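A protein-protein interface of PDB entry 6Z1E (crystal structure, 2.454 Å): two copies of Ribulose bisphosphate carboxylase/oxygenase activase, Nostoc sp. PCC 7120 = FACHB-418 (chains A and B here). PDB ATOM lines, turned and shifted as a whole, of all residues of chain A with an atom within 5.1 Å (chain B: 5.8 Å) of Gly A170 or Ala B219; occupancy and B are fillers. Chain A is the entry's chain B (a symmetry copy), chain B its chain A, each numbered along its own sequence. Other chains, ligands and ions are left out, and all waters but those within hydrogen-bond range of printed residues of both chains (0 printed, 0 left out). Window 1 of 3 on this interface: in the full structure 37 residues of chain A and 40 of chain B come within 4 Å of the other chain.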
ATOM      1  N   ARG A  27     -11.308  -8.423   1.753  1.00  0.00           N
ATOM      2  CA  ARG A  27     -12.596  -8.023   1.199  1.00  0.00           C
ATOM      3  C   ARG A  27     -12.672  -6.509   1.121  1.00  0.00           C
ATOM      4  O   ARG A  27     -12.262  -5.806   2.040  1.00  0.00           O
ATOM      5  CB  ARG A  27     -13.741  -8.560   2.050  1.00  0.00           C
ATOM      6  CG  ARG A  27     -15.112  -8.368   1.429  1.00  0.00           C
ATOM      7  CD  ARG A  27     -16.164  -9.143   2.197  1.00  0.00           C
ATOM      8  NE  ARG A  27     -16.089  -8.875   3.630  1.00  0.00           N
ATOM      9  CZ  ARG A  27     -16.605  -7.803   4.224  1.00  0.00           C
ATOM     10  NH1 ARG A  27     -17.243  -6.881   3.513  1.00  0.00           N
ATOM     11  NH2 ARG A  27     -16.481  -7.651   5.535  1.00  0.00           N
ATOM     12  N   VAL A  28     -13.211  -6.019   0.015  1.00  0.00           N
ATOM     13  CA  VAL A  28     -13.170  -4.604  -0.311  1.00  0.00           C
ATOM     14  C   VAL A  28     -14.578  -4.019  -0.284  1.00  0.00           C
ATOM     15  O   VAL A  28     -15.540  -4.695  -0.653  1.00  0.00           O
ATOM     16  CB  VAL A  28     -12.550  -4.409  -1.711  1.00  0.00           C
ATOM     17  CG1 VAL A  28     -12.608  -2.956  -2.149  1.00  0.00           C
ATOM     18  CG2 VAL A  28     -11.114  -4.913  -1.716  1.00  0.00           C
ATOM     19  N   PRO A  29     -14.714  -2.761   0.165  1.00  0.00           N
ATOM     20  CA  PRO A  29     -16.016  -2.096   0.040  1.00  0.00           C
ATOM     21  C   PRO A  29     -16.277  -1.662  -1.402  1.00  0.00           C
ATOM     22  O   PRO A  29     -15.377  -1.130  -2.049  1.00  0.00           O
ATOM     23  CB  PRO A  29     -15.873  -0.874   0.949  1.00  0.00           C
ATOM     24  CG  PRO A  29     -14.412  -0.598   0.991  1.00  0.00           C
ATOM     25  CD  PRO A  29     -13.738  -1.933   0.898  1.00  0.00           C
ATOM     26  N   PRO A 165     -25.699  -0.252   8.188  1.00  0.00           N
ATOM     27  CA  PRO A 165     -25.363  -1.667   7.981  1.00  0.00           C
ATOM     28  C   PRO A 165     -24.277  -1.881   6.927  1.00  0.00           C
ATOM     29  O   PRO A 165     -23.412  -2.735   7.103  1.00  0.00           O
ATOM     30  CB  PRO A 165     -26.687  -2.271   7.504  1.00  0.00           C
ATOM     31  CG  PRO A 165     -27.724  -1.413   8.114  1.00  0.00           C
ATOM     32  CD  PRO A 165     -27.154  -0.027   8.118  1.00  0.00           C
ATOM     33  N   LEU A 166     -24.328  -1.111   5.847  1.00  0.00           N
ATOM     34  CA  LEU A 166     -23.323  -1.189   4.793  1.00  0.00           C
ATOM     35  C   LEU A 166     -21.941  -0.812   5.306  1.00  0.00           C
ATOM     36  O   LEU A 166     -20.945  -1.449   4.963  1.00  0.00           O
ATOM     37  CB  LEU A 166     -23.689  -0.260   3.631  1.00  0.00           C
ATOM     38  CG  LEU A 166     -24.644  -0.818   2.580  1.00  0.00           C
ATOM     39  CD1 LEU A 166     -25.054   0.272   1.604  1.00  0.00           C
ATOM     40  CD2 LEU A 166     -23.994  -1.968   1.839  1.00  0.00           C
ATOM     41  N   ILE A 167     -21.889   0.232   6.124  1.00  0.00           N
ATOM     42  CA  ILE A 167     -20.624   0.752   6.621  1.00  0.00           C
ATOM     43  C   ILE A 167     -20.028  -0.192   7.666  1.00  0.00           C
ATOM     44  O   ILE A 167     -18.817  -0.410   7.696  1.00  0.00           O
ATOM     45  CB  ILE A 167     -20.807   2.174   7.196  1.00  0.00           C
ATOM     46  CG1 ILE A 167     -21.284   3.123   6.089  1.00  0.00           C
ATOM     47  CG2 ILE A 167     -19.505   2.696   7.795  1.00  0.00           C
ATOM     48  CD1 ILE A 167     -21.900   4.408   6.595  1.00  0.00           C
ATOM     49  N   ARG A 168     -20.885  -0.757   8.511  1.00  0.00           N
ATOM     50  CA  ARG A 168     -20.449  -1.710   9.530  1.00  0.00           C
ATOM     51  C   ARG A 168     -19.872  -2.981   8.925  1.00  0.00           C
ATOM     52  O   ARG A 168     -18.862  -3.495   9.398  1.00  0.00           O
ATOM     53  CB  ARG A 168     -21.618  -2.084  10.435  1.00  0.00           C
ATOM     54  CG  ARG A 168     -21.796  -1.161  11.614  1.00  0.00           C
ATOM     55  CD  ARG A 168     -23.177  -1.297  12.208  1.00  0.00           C
ATOM     56  NE  ARG A 168     -23.633  -0.035  12.779  1.00  0.00           N
ATOM     57  CZ  ARG A 168     -24.909   0.298  12.935  1.00  0.00           C
ATOM     58  NH1 ARG A 168     -25.875  -0.533  12.561  1.00  0.00           N
ATOM     59  NH2 ARG A 168     -25.223   1.474  13.462  1.00  0.00           N
ATOM     60  N   ASP A 169     -20.527  -3.491   7.888  1.00  0.00           N
ATOM     61  CA  ASP A 169     -20.121  -4.743   7.262  1.00  0.00           C
ATOM     62  C   ASP A 169     -19.015  -4.531   6.234  1.00  0.00           C
ATOM     63  O   ASP A 169     -18.603  -5.470   5.557  1.00  0.00           O
ATOM     64  CB  ASP A 169     -21.326  -5.417   6.601  1.00  0.00           C
ATOM     65  CG  ASP A 169     -22.282  -6.026   7.610  1.00  0.00           C
ATOM     66  OD1 ASP A 169     -22.094  -5.807   8.827  1.00  0.00           O
ATOM     67  OD2 ASP A 169     -23.226  -6.724   7.183  1.00  0.00           O
ATOM     68  N   GLY A 170     -18.528  -3.299   6.125  1.00  0.00           N
ATOM     69  CA  GLY A 170     -17.461  -2.983   5.193  1.00  0.00           C
ATOM     70  C   GLY A 170     -17.855  -3.178   3.741  1.00  0.00           C
ATOM     71  O   GLY A 170     -17.046  -3.617   2.927  1.00  0.00           O
ATOM     72  N   ARG A 171     -19.106  -2.865   3.422  1.00  0.00           N
ATOM     73  CA  ARG A 171     -19.579  -2.890   2.044  1.00  0.00           C
ATOM     74  C   ARG A 171     -19.585  -1.473   1.494  1.00  0.00           C
ATOM     75  O   ARG A 171     -19.715  -1.261   0.289  1.00  0.00           O
ATOM     76  CB  ARG A 171     -20.989  -3.464   1.974  1.00  0.00           C
ATOM     77  CG  ARG A 171     -21.150  -4.826   2.623  1.00  0.00           C
ATOM     78  CD  ARG A 171     -21.223  -5.939   1.593  1.00  0.00           C
ATOM     79  NE  ARG A 171     -21.801  -7.158   2.164  1.00  0.00           N
ATOM     80  CZ  ARG A 171     -21.111  -8.215   2.581  1.00  0.00           C
ATOM     81  NH1 ARG A 171     -21.755  -9.260   3.083  1.00  0.00           N
ATOM     82  NH2 ARG A 171     -19.786  -8.242   2.496  1.00  0.00           N
ATOM     83  N   MET A 172     -19.443  -0.502   2.390  1.00  0.00           N
ATOM     84  CA  MET A 172     -19.406   0.899   2.014  1.00  0.00           C
ATOM     85  C   MET A 172     -18.434   1.646   2.912  1.00  0.00           C
ATOM     86  O   MET A 172     -18.426   1.453   4.122  1.00  0.00           O
ATOM     87  CB  MET A 172     -20.792   1.516   2.159  1.00  0.00           C
ATOM     88  CG  MET A 172     -20.828   3.006   1.900  1.00  0.00           C
ATOM     89  SD  MET A 172     -22.490   3.667   2.024  1.00  0.00           S
ATOM     90  CE  MET A 172     -22.167   5.373   1.611  1.00  0.00           C
ATOM     91  N   ILE B 214     -19.731 -10.785  11.814  1.00  0.00           N
ATOM     92  CA  ILE B 214     -18.456 -11.332  11.370  1.00  0.00           C
ATOM     93  C   ILE B 214     -17.845 -10.467  10.271  1.00  0.00           C
ATOM     94  O   ILE B 214     -16.634 -10.262  10.241  1.00  0.00           O
ATOM     95  CB  ILE B 214     -18.630 -12.781  10.861  1.00  0.00           C
ATOM     96  CG1 ILE B 214     -19.172 -13.674  11.983  1.00  0.00           C
ATOM     97  CG2 ILE B 214     -17.317 -13.339  10.325  1.00  0.00           C
ATOM     98  CD1 ILE B 214     -18.311 -13.703  13.239  1.00  0.00           C
ATOM     99  N   ASP B 215     -18.681  -9.952   9.377  1.00  0.00           N
ATOM    100  CA  ASP B 215     -18.197  -9.130   8.273  1.00  0.00           C
ATOM    101  C   ASP B 215     -17.537  -7.837   8.756  1.00  0.00           C
ATOM    102  O   ASP B 215     -16.656  -7.303   8.086  1.00  0.00           O
ATOM    103  CB  ASP B 215     -19.334  -8.813   7.295  1.00  0.00           C
ATOM    104  CG  ASP B 215     -19.605  -9.949   6.323  1.00  0.00           C
ATOM    105  OD1 ASP B 215     -19.107 -11.070   6.564  1.00  0.00           O
ATOM    106  OD2 ASP B 215     -20.321  -9.720   5.323  1.00  0.00           O
ATOM    107  N   PHE B 216     -17.961  -7.339   9.914  1.00  0.00           N
ATOM    108  CA  PHE B 216     -17.369  -6.133  10.488  1.00  0.00           C
ATOM    109  C   PHE B 216     -15.885  -6.328  10.775  1.00  0.00           C
ATOM    110  O   PHE B 216     -15.087  -5.412  10.595  1.00  0.00           O
ATOM    111  CB  PHE B 216     -18.098  -5.723  11.776  1.00  0.00           C
ATOM    112  CG  PHE B 216     -17.357  -4.705  12.597  1.00  0.00           C
ATOM    113  CD1 PHE B 216     -17.501  -3.351  12.346  1.00  0.00           C
ATOM    114  CD2 PHE B 216     -16.515  -5.103  13.625  1.00  0.00           C
ATOM    115  CE1 PHE B 216     -16.818  -2.415  13.100  1.00  0.00           C
ATOM    116  CE2 PHE B 216     -15.828  -4.171  14.379  1.00  0.00           C
ATOM    117  CZ  PHE B 216     -15.980  -2.826  14.117  1.00  0.00           C
ATOM    118  N   PHE B 217     -15.524  -7.531  11.209  1.00  0.00           N
ATOM    119  CA  PHE B 217     -14.157  -7.814  11.633  1.00  0.00           C
ATOM    120  C   PHE B 217     -13.227  -8.077  10.454  1.00  0.00           C
ATOM    121  O   PHE B 217     -12.062  -7.682  10.476  1.00  0.00           O
ATOM    122  CB  PHE B 217     -14.140  -9.007  12.587  1.00  0.00           C
ATOM    123  CG  PHE B 217     -14.854  -8.749  13.881  1.00  0.00           C
ATOM    124  CD1 PHE B 217     -14.204  -8.124  14.932  1.00  0.00           C
ATOM    125  CD2 PHE B 217     -16.177  -9.120  14.043  1.00  0.00           C
ATOM    126  CE1 PHE B 217     -14.860  -7.878  16.122  1.00  0.00           C
ATOM    127  CE2 PHE B 217     -16.838  -8.880  15.231  1.00  0.00           C
ATOM    128  CZ  PHE B 217     -16.179  -8.257  16.273  1.00  0.00           C
ATOM    129  N   SER B 218     -13.737  -8.749   9.428  1.00  0.00           N
ATOM    130  CA  SER B 218     -12.945  -8.993   8.230  1.00  0.00           C
ATOM    131  C   SER B 218     -12.724  -7.687   7.481  1.00  0.00           C
ATOM    132  O   SER B 218     -11.669  -7.472   6.884  1.00  0.00           O
ATOM    133  CB  SER B 218     -13.630 -10.014   7.323  1.00  0.00           C
ATOM    134  OG  SER B 218     -14.942  -9.601   6.994  1.00  0.00           O
ATOM    135  N   ALA B 219     -13.724  -6.813   7.523  1.00  0.00           N
ATOM    136  CA  ALA B 219     -13.620  -5.500   6.899  1.00  0.00           C
ATOM    137  C   ALA B 219     -12.578  -4.680   7.634  1.00  0.00           C
ATOM    138  O   ALA B 219     -11.877  -3.862   7.041  1.00  0.00           O
ATOM    139  CB  ALA B 219     -14.951  -4.789   6.940  1.00  0.00           C
ATOM    140  N   LEU B 220     -12.498  -4.900   8.937  1.00  0.00           N
ATOM    141  CA  LEU B 220     -11.552  -4.190   9.779  1.00  0.00           C
ATOM    142  C   LEU B 220     -10.132  -4.505   9.334  1.00  0.00           C
ATOM    143  O   LEU B 220      -9.273  -3.627   9.300  1.00  0.00           O
ATOM    144  CB  LEU B 220     -11.755  -4.595  11.241  1.00  0.00           C
ATOM    145  CG  LEU B 220     -11.128  -3.716  12.321  1.00  0.00           C
ATOM    146  CD1 LEU B 220     -11.650  -2.287  12.249  1.00  0.00           C
ATOM    147  CD2 LEU B 220     -11.418  -4.329  13.678  1.00  0.00           C
ATOM    148  N   ARG B 221      -9.893  -5.765   8.985  1.00  0.00           N
ATOM    149  CA  ARG B 221      -8.566  -6.207   8.574  1.00  0.00           C
ATOM    150  C   ARG B 221      -8.183  -5.689   7.193  1.00  0.00           C
ATOM    151  O   ARG B 221      -7.019  -5.387   6.935  1.00  0.00           O
ATOM    152  CB  ARG B 221      -8.494  -7.735   8.561  1.00  0.00           C
ATOM    153  CG  ARG B 221      -7.078  -8.272   8.415  1.00  0.00           C
ATOM    154  CD  ARG B 221      -7.037  -9.788   8.354  1.00  0.00           C
ATOM    155  NE  ARG B 221      -5.661 -10.279   8.307  1.00  0.00           N
ATOM    156  CZ  ARG B 221      -4.915 -10.327   7.207  1.00  0.00           C
ATOM    157  NH1 ARG B 221      -5.403  -9.916   6.045  1.00  0.00           N
ATOM    158  NH2 ARG B 221      -3.674 -10.788   7.270  1.00  0.00           N
ATOM    159  N   SER B 222      -9.169  -5.589   6.311  1.00  0.00           N
ATOM    160  CA  SER B 222      -8.914  -5.314   4.902  1.00  0.00           C
ATOM    161  C   SER B 222      -8.426  -3.893   4.647  1.00  0.00           C
ATOM    162  O   SER B 222      -7.662  -3.655   3.713  1.00  0.00           O
ATOM    163  CB  SER B 222     -10.185  -5.566   4.088  1.00  0.00           C
ATOM    164  OG  SER B 222     -10.648  -6.892   4.265  1.00  0.00           O
ATOM    165  N   ARG B 223      -8.863  -2.953   5.476  1.00  0.00           N
ATOM    166  CA  ARG B 223      -8.580  -1.542   5.235  1.00  0.00           C
ATOM    167  C   ARG B 223      -7.130  -1.165   5.539  1.00  0.00           C
ATOM    168  O   ARG B 223      -6.704  -0.050   5.243  1.00  0.00           O
ATOM    169  CB  ARG B 223      -9.530  -0.661   6.052  1.00  0.00           C
ATOM    170  CG  ARG B 223      -9.382  -0.818   7.551  1.00  0.00           C
ATOM    171  CD  ARG B 223     -10.555  -0.205   8.290  1.00  0.00           C
ATOM    172  NE  ARG B 223     -10.839   1.148   7.816  1.00  0.00           N
ATOM    173  CZ  ARG B 223     -11.924   1.515   7.135  1.00  0.00           C
ATOM    174  NH1 ARG B 223     -12.877   0.640   6.834  1.00  0.00           N
ATOM    175  NH2 ARG B 223     -12.065   2.780   6.758  1.00  0.00           N
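No position is printed for both chains.
Of the 9 pairs that touch across the chains among the printed residues, none has its exchanged pair printed and touching as well.
Of the printed residues of chain B, Asp A169 touches Asp B215 (3.7 Å) and Ala B219 (3.96 Å).
Of the printed residues of chain B, Gly A170 touches Ala B219.
Of chain A, only Arg A27, Asp A169 and Gly A170 come within 4 Å of Ala B219.
Arg B221 touches none of the printed residues of chain A.
Printed residues of chain A within 4 Å of Ser B222: Arg A27 (2.9 Å).
The guanidinium group (NH1) of Arg A27 is in hydrogen-bond range of the backbone carbonyl oxygen (O) of Asp A169 (2.8 Å).
The backbone carbonyl oxygen (O) of Asp B215 is in hydrogen-bond range of the side-chain hydroxyl (OG) of Ser B218.
O of Gly A170 is in hydrogen-bond range of NH1 of Arg A27 (3.3 Å).
O of Ser B218 sits at hydrogen-bond distance from OG of Ser B222 (2.9 Å).
N of Arg A171 is in hydrogen-bond range of O of Leu A166 (2.8 Å).
Ala B219 touches Arg A27 (N to NH2, 3.5 Å).
O of Arg A168 touches CA of Phe B216, 3.2 Å away.
Asp B215 touches Asp A169 (O to O, 3.7 Å).
O of Asp A169 touches CB of Ala B219, 3.96 Å away.
Gly A170 touches Ala B219.
Of the 11 printed residues of chain A, 5 touch a printed residue of chain B.
Printed residues of chain A that touch a printed residue of chain B: Arg A27, Arg A168, Asp A169, Gly A170 and Arg A171.
Printed residues of chain B that touch a printed residue of chain A: Asp B215, Phe B216, Ser B218, Ala B219 and Ser B222.
Hydrophobic or aromatic side chains of chain B that line the printed part of chain A: Phe B216 and Ala B219.
The backbone carbonyl oxygen (O) of Arg A27 lies close to the side-chain hydroxyl (OG) of Ser B222 (3.0 Å).
NH2 of Arg A27 lies within hydrogen-bond range of OG of Ser B218, 2.9 Å away.
The side-chain carboxylate of Asp B215 lies within salt-bridge range of the guanidinium group of Arg A171.
The guanidinium group of Arg A27 is in hydrogen-bond range of the backbone carbonyl oxygen of Asp B215 (2.6 Å).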
